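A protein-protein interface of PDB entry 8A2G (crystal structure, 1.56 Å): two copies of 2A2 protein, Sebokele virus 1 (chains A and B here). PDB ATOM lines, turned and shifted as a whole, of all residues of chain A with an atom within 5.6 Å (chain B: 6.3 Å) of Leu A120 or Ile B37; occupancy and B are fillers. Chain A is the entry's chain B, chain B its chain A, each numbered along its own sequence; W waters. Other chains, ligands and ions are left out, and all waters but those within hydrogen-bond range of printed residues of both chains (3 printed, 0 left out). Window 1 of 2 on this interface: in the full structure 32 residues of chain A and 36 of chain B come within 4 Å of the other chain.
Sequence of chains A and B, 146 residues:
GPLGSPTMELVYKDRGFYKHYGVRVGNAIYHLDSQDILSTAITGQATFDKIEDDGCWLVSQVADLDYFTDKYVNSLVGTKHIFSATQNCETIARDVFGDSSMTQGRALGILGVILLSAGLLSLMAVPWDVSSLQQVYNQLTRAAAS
The backbone carbonyl oxygen (O) of Asp B36 is in hydrogen-bond range of the side-chain hydroxyl (OG1) of Thr B40 (3.1 Å).
OD2 of Asp B36 sits at hydrogen-bond distance from OG of Ser B39, 2.9 Å away.
The side-chain hydroxyl (OG) of Ser B34 lies within hydrogen-bond range of the backbone NH (N) of Asp B36, at 3.0 Å.
Water W2 lies within hydrogen-bond range of the backbone carbonyl oxygen (O) of Leu A123 (2.6 Å) and the backbone carbonyl oxygen (O) of Leu B123 (3.0 Å).
Water W1 lies within hydrogen-bond range of the backbone carbonyl oxygen (O) of Leu A123 (2.8 Å) and the backbone carbonyl oxygen (O) of Leu B123 (3.2 Å).
Water W3 lies within hydrogen-bond range of O of Leu A140, N of Gln B35 and N of Asp B36.
Positions printed for both chains: 116 and 123.
The backbone NH of Asp B36 sits at hydrogen-bond distance from the backbone carbonyl oxygen of Leu A140.
Of the 12 printed residues of chain A, 4 touch a printed residue of chain B.
Among the printed residues, no Asp or Glu carboxylate lies within 4 Å of a Lys or Arg side-chain nitrogen of the other chain.
Leu A116 touches Leu B38.
Leu B38 touches Ser A117.
Ile B37 touches Leu A120.
CG of Leu B38 touches CD2 of Leu A120, 3.6 Å away.
O of Leu A140 touches C of Gln B35, at 3.3 Å.
Printed residues of chain B within 4 Å of Ser A117: Leu B38 (3.6 Å).
Printed residues of chain B within 4 Å of Leu A120: Ile B37 (3.7 Å) and Leu B38 (3.6 Å).
Of the printed residues of chain B, Leu A140 touches Gln B35 and Asp B36.
Leu B32 touches none of the printed residues of chain A.
Ile B37 touches just one residue of chain A: Leu A120 (3.7 Å).
The nearest residue of chain A that does not touch Ile B37 is Leu A140 (4.1 Å).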
ATOM      1  N   LEU A 115      17.545 -34.591  19.166  1.00  0.00           N
ATOM      2  CA  LEU A 115      16.852 -34.287  20.399  1.00  0.00           C
ATOM      3  C   LEU A 115      17.636 -33.260  21.237  1.00  0.00           C
ATOM      4  O   LEU A 115      17.025 -32.381  21.852  1.00  0.00           O
ATOM      5  CB  LEU A 115      16.587 -35.573  21.197  1.00  0.00           C
ATOM      6  CG  LEU A 115      15.734 -36.609  20.476  1.00  0.00           C
ATOM      7  CD1 LEU A 115      15.451 -37.749  21.412  1.00  0.00           C
ATOM      8  CD2 LEU A 115      14.431 -35.986  19.954  1.00  0.00           C
ATOM      9  N   LEU A 116      18.961 -33.374  21.300  1.00  0.00           N
ATOM     10  CA  LEU A 116      19.709 -32.388  22.083  1.00  0.00           C
ATOM     11  C   LEU A 116      19.676 -31.033  21.385  1.00  0.00           C
ATOM     12  O   LEU A 116      19.604 -30.006  22.049  1.00  0.00           O
ATOM     13  CB  LEU A 116      21.162 -32.802  22.345  1.00  0.00           C
ATOM     14  CG  LEU A 116      21.380 -34.025  23.228  1.00  0.00           C
ATOM     15  CD1 LEU A 116      22.849 -34.090  23.640  1.00  0.00           C
ATOM     16  CD2 LEU A 116      20.485 -34.043  24.441  1.00  0.00           C
ATOM     17  N   SER A 117      19.753 -30.998  20.053  1.00  0.00           N
ATOM     18  CA  SER A 117      19.631 -29.747  19.307  1.00  0.00           C
ATOM     19  C   SER A 117      18.292 -29.062  19.582  1.00  0.00           C
ATOM     20  O   SER A 117      18.208 -27.876  19.907  1.00  0.00           O
ATOM     21  CB  SER A 117      19.813 -29.984  17.821  1.00  0.00           C
ATOM     22  OG  SER A 117      21.125 -30.408  17.439  1.00  0.00           O
ATOM     23  N   ALA A 118      17.209 -29.819  19.473  1.00  0.00           N
ATOM     24  CA  ALA A 118      15.891 -29.268  19.727  1.00  0.00           C
ATOM     25  C   ALA A 118      15.803 -28.720  21.152  1.00  0.00           C
ATOM     26  O   ALA A 118      15.260 -27.645  21.393  1.00  0.00           O
ATOM     27  CB  ALA A 118      14.829 -30.322  19.449  1.00  0.00           C
ATOM     28  N   GLY A 119      16.295 -29.506  22.105  1.00  0.00           N
ATOM     29  CA  GLY A 119      16.223 -29.083  23.487  1.00  0.00           C
ATOM     30  C   GLY A 119      17.051 -27.836  23.780  1.00  0.00           C
ATOM     31  O   GLY A 119      16.589 -26.954  24.477  1.00  0.00           O
ATOM     32  N   LEU A 120      18.249 -27.766  23.232  1.00  0.00           N
ATOM     33  CA  LEU A 120      19.115 -26.602  23.445  1.00  0.00           C
ATOM     34  C   LEU A 120      18.519 -25.374  22.769  1.00  0.00           C
ATOM     35  O   LEU A 120      18.502 -24.284  23.358  1.00  0.00           O
ATOM     36  CB  LEU A 120      20.511 -26.887  22.892  1.00  0.00           C
ATOM     37  CG  LEU A 120      21.511 -25.751  23.078  1.00  0.00           C
ATOM     38  CD1 LEU A 120      21.715 -25.496  24.565  1.00  0.00           C
ATOM     39  CD2 LEU A 120      22.826 -26.044  22.381  1.00  0.00           C
ATOM     40  N   LEU A 121      18.059 -25.521  21.523  1.00  0.00           N
ATOM     41  CA  LEU A 121      17.493 -24.385  20.818  1.00  0.00           C
ATOM     42  C   LEU A 121      16.249 -23.880  21.544  1.00  0.00           C
ATOM     43  O   LEU A 121      16.046 -22.678  21.622  1.00  0.00           O
ATOM     44  CB  LEU A 121      17.208 -24.783  19.371  1.00  0.00           C
ATOM     45  CG  LEU A 121      18.445 -25.001  18.511  1.00  0.00           C
ATOM     46  CD1 LEU A 121      18.081 -25.749  17.237  1.00  0.00           C
ATOM     47  CD2 LEU A 121      19.142 -23.679  18.185  1.00  0.00           C
ATOM     48  N   SER A 122      15.416 -24.781  22.081  1.00  0.00           N
ATOM     49  CA  SER A 122      14.270 -24.378  22.870  1.00  0.00           C
ATOM     50  C   SER A 122      14.709 -23.588  24.107  1.00  0.00           C
ATOM     51  O   SER A 122      14.119 -22.557  24.447  1.00  0.00           O
ATOM     52  CB  SER A 122      13.442 -25.586  23.232  1.00  0.00           C
ATOM     53  OG  SER A 122      12.386 -25.228  24.097  1.00  0.00           O
ATOM     54  N   LEU A 123      15.739 -24.048  24.808  1.00  0.00           N
ATOM     55  CA  LEU A 123      16.218 -23.319  25.980  1.00  0.00           C
ATOM     56  C   LEU A 123      16.640 -21.903  25.603  1.00  0.00           C
ATOM     57  O   LEU A 123      16.458 -20.980  26.396  1.00  0.00           O
ATOM     58  CB  LEU A 123      17.389 -24.048  26.624  1.00  0.00           C
ATOM     59  CG  LEU A 123      16.998 -25.204  27.526  1.00  0.00           C
ATOM     60  CD1 LEU A 123      18.258 -25.854  28.064  1.00  0.00           C
ATOM     61  CD2 LEU A 123      16.111 -24.689  28.659  1.00  0.00           C
ATOM     62  N   MET A 124      17.206 -21.753  24.409  1.00  0.00           N
ATOM     63  CA  MET A 124      17.668 -20.451  23.934  1.00  0.00           C
ATOM     64  C   MET A 124      16.562 -19.625  23.299  1.00  0.00           C
ATOM     65  O   MET A 124      16.807 -18.473  22.934  1.00  0.00           O
ATOM     66  CB  MET A 124      18.726 -20.675  22.861  1.00  0.00           C
ATOM     67  CG  MET A 124      19.939 -21.185  23.387  1.00  0.00           C
ATOM     68  SD  MET A 124      20.950 -21.511  21.934  1.00  0.00           S
ATOM     69  CE  MET A 124      22.441 -21.840  22.759  1.00  0.00           C
ATOM     70  N   ALA A 125      15.378 -20.216  23.105  1.00  0.00           N
ATOM     71  CA  ALA A 125      14.242 -19.594  22.456  1.00  0.00           C
ATOM     72  C   ALA A 125      14.644 -19.084  21.075  1.00  0.00           C
ATOM     73  O   ALA A 125      14.268 -17.982  20.672  1.00  0.00           O
ATOM     74  CB  ALA A 125      13.707 -18.487  23.339  1.00  0.00           C
ATOM     75  N   LEU A 140      28.081 -20.892  18.510  1.00  0.00           N
ATOM     76  CA  LEU A 140      28.493 -22.159  19.102  1.00  0.00           C
ATOM     77  C   LEU A 140      29.886 -22.560  18.615  1.00  0.00           C
ATOM     78  O   LEU A 140      30.676 -23.154  19.356  1.00  0.00           O
ATOM     79  CB  LEU A 140      27.473 -23.252  18.781  1.00  0.00           C
ATOM     80  CG  LEU A 140      26.159 -23.215  19.563  1.00  0.00           C
ATOM     81  CD1 LEU A 140      25.143 -24.221  18.997  1.00  0.00           C
ATOM     82  CD2 LEU A 140      26.389 -23.471  21.054  1.00  0.00           C
ATOM     83  N   LEU B  32      36.564 -24.291  29.074  1.00  0.00           N
ATOM     84  CA  LEU B  32      36.522 -25.313  28.033  1.00  0.00           C
ATOM     85  C   LEU B  32      36.937 -24.705  26.702  1.00  0.00           C
ATOM     86  O   LEU B  32      36.513 -23.601  26.339  1.00  0.00           O
ATOM     87  CB  LEU B  32      35.114 -25.906  28.007  1.00  0.00           C
ATOM     88  CG  LEU B  32      34.668 -26.589  29.293  1.00  0.00           C
ATOM     89  CD1 LEU B  32      33.256 -27.173  29.136  1.00  0.00           C
ATOM     90  CD2 LEU B  32      35.634 -27.659  29.729  1.00  0.00           C
ATOM     91  N   SER B  34      36.302 -25.478  23.695  1.00  0.00           N
ATOM     92  CA  SER B  34      35.236 -25.357  22.719  1.00  0.00           C
ATOM     93  C   SER B  34      34.003 -24.814  23.440  1.00  0.00           C
ATOM     94  O   SER B  34      33.683 -25.271  24.545  1.00  0.00           O
ATOM     95  CB  SER B  34      34.918 -26.679  22.074  1.00  0.00           C
ATOM     96  OG  SER B  34      33.753 -26.592  21.242  1.00  0.00           O
ATOM     97  N   GLN B  35      33.275 -23.905  22.788  1.00  0.00           N
ATOM     98  CA  GLN B  35      31.988 -23.478  23.315  1.00  0.00           C
ATOM     99  C   GLN B  35      30.852 -24.116  22.527  1.00  0.00           C
ATOM    100  O   GLN B  35      29.685 -23.739  22.667  1.00  0.00           O
ATOM    101  CB  GLN B  35      31.936 -21.951  23.393  1.00  0.00           C
ATOM    102  CG  GLN B  35      32.159 -21.226  22.081  1.00  0.00           C
ATOM    103  CD  GLN B  35      32.242 -19.751  22.393  1.00  0.00           C
ATOM    104  OE1 GLN B  35      32.070 -19.333  23.542  1.00  0.00           O
ATOM    105  NE2 GLN B  35      32.665 -18.993  21.407  1.00  0.00           N
ATOM    106  N   ASP B  36      31.179 -25.115  21.711  1.00  0.00           N
ATOM    107  CA  ASP B  36      30.184 -25.898  20.990  1.00  0.00           C
ATOM    108  C   ASP B  36      29.653 -26.953  21.956  1.00  0.00           C
ATOM    109  O   ASP B  36      30.057 -28.107  21.923  1.00  0.00           O
ATOM    110  CB  ASP B  36      30.762 -26.503  19.719  1.00  0.00           C
ATOM    111  CG  ASP B  36      29.720 -27.161  18.825  1.00  0.00           C
ATOM    112  OD1 ASP B  36      28.538 -27.226  19.259  1.00  0.00           O
ATOM    113  OD2 ASP B  36      30.116 -27.633  17.752  1.00  0.00           O
ATOM    114  N   ILE B  37      28.713 -26.530  22.790  1.00  0.00           N
ATOM    115  CA  ILE B  37      28.244 -27.384  23.863  1.00  0.00           C
ATOM    116  C   ILE B  37      27.518 -28.591  23.295  1.00  0.00           C
ATOM    117  O   ILE B  37      27.513 -29.647  23.929  1.00  0.00           O
ATOM    118  CB  ILE B  37      27.352 -26.609  24.842  1.00  0.00           C
ATOM    119  CG1 ILE B  37      27.036 -27.439  26.091  1.00  0.00           C
ATOM    120  CG2 ILE B  37      26.092 -26.179  24.123  1.00  0.00           C
ATOM    121  CD1 ILE B  37      28.249 -28.036  26.791  1.00  0.00           C
ATOM    122  N   LEU B  38      26.899 -28.474  22.115  1.00  0.00           N
ATOM    123  CA  LEU B  38      26.320 -29.646  21.493  1.00  0.00           C
ATOM    124  C   LEU B  38      27.372 -30.693  21.166  1.00  0.00           C
ATOM    125  O   LEU B  38      27.149 -31.856  21.487  1.00  0.00           O
ATOM    126  CB  LEU B  38      25.535 -29.282  20.229  1.00  0.00           C
ATOM    127  CG  LEU B  38      24.124 -28.835  20.517  1.00  0.00           C
ATOM    128  CD1 LEU B  38      23.475 -28.315  19.250  1.00  0.00           C
ATOM    129  CD2 LEU B  38      23.319 -29.979  21.136  1.00  0.00           C
ATOM    130  N   SER B  39      28.482 -30.311  20.521  1.00  0.00           N
ATOM    131  CA  SER B  39      29.520 -31.269  20.188  1.00  0.00           C
ATOM    132  C   SER B  39      30.085 -31.878  21.466  1.00  0.00           C
ATOM    133  O   SER B  39      30.268 -33.088  21.558  1.00  0.00           O
ATOM    134  CB  SER B  39      30.599 -30.623  19.367  1.00  0.00           C
ATOM    135  OG  SER B  39      30.186 -30.567  18.015  1.00  0.00           O
ATOM    136  N   THR B  40      30.300 -31.020  22.464  1.00  0.00           N
ATOM    137  CA  THR B  40      30.803 -31.455  23.753  1.00  0.00           C
ATOM    138  C   THR B  40      29.861 -32.491  24.372  1.00  0.00           C
ATOM    139  O   THR B  40      30.292 -33.562  24.798  1.00  0.00           O
ATOM    140  CB  THR B  40      30.946 -30.262  24.699  1.00  0.00           C
ATOM    141  OG1 THR B  40      31.880 -29.339  24.132  1.00  0.00           O
ATOM    142  CG2 THR B  40      31.404 -30.674  26.080  1.00  0.00           C
ATOM    143  N   ALA B  41      28.552 -32.188  24.400  1.00  0.00           N
ATOM    144  CA  ALA B  41      27.569 -33.066  25.031  1.00  0.00           C
ATOM    145  C   ALA B  41      27.442 -34.374  24.235  1.00  0.00           C
ATOM    146  O   ALA B  41      27.427 -35.443  24.842  1.00  0.00           O
ATOM    147  CB  ALA B  41      26.217 -32.391  25.172  1.00  0.00           C
ATOM    148  N   ILE B  42      27.364 -34.300  22.894  1.00  0.00           N
ATOM    149  CA  ILE B  42      27.137 -35.465  22.047  1.00  0.00           C
ATOM    150  C   ILE B  42      28.333 -36.419  22.092  1.00  0.00           C
ATOM    151  O   ILE B  42      28.151 -37.633  22.101  1.00  0.00           O
ATOM    152  CB  ILE B  42      26.805 -35.038  20.607  1.00  0.00           C
ATOM    153  CG1 ILE B  42      25.454 -34.313  20.503  1.00  0.00           C
ATOM    154  CG2 ILE B  42      26.844 -36.243  19.678  1.00  0.00           C
ATOM    155  CD1 ILE B  42      25.328 -33.440  19.267  1.00  0.00           C
ATOM    156  N   LEU B 116      29.555 -25.891  33.682  1.00  0.00           N
ATOM    157  CA  LEU B 116      28.346 -26.327  32.989  1.00  0.00           C
ATOM    158  C   LEU B 116      27.111 -25.880  33.787  1.00  0.00           C
ATOM    159  O   LEU B 116      26.077 -25.486  33.209  1.00  0.00           O
ATOM    160  CB  LEU B 116      28.299 -27.832  32.727  1.00  0.00           C
ATOM    161  CG  LEU B 116      29.330 -28.376  31.729  1.00  0.00           C
ATOM    162  CD1 LEU B 116      28.934 -29.800  31.340  1.00  0.00           C
ATOM    163  CD2 LEU B 116      29.488 -27.488  30.517  1.00  0.00           C
ATOM    164  N   LEU B 123      21.041 -19.931  31.269  1.00  0.00           N
ATOM    165  CA  LEU B 123      20.051 -20.098  30.218  1.00  0.00           C
ATOM    166  C   LEU B 123      18.647 -20.173  30.802  1.00  0.00           C
ATOM    167  O   LEU B 123      17.686 -19.758  30.153  1.00  0.00           O
ATOM    168  CB  LEU B 123      20.322 -21.361  29.423  1.00  0.00           C
ATOM    169  CG  LEU B 123      21.503 -21.321  28.464  1.00  0.00           C
ATOM    170  CD1 LEU B 123      21.683 -22.667  27.802  1.00  0.00           C
ATOM    171  CD2 LEU B 123      21.289 -20.238  27.415  1.00  0.00           C
HETATM  172  O   HOH W   1      15.043 -21.011  28.761  1.00  0.00           O
HETATM  173  O   HOH W   2      17.601 -18.788  27.322  1.00  0.00           O
HETATM  174  O   HOH W   3      33.464 -23.254  19.908  1.00  0.00           O
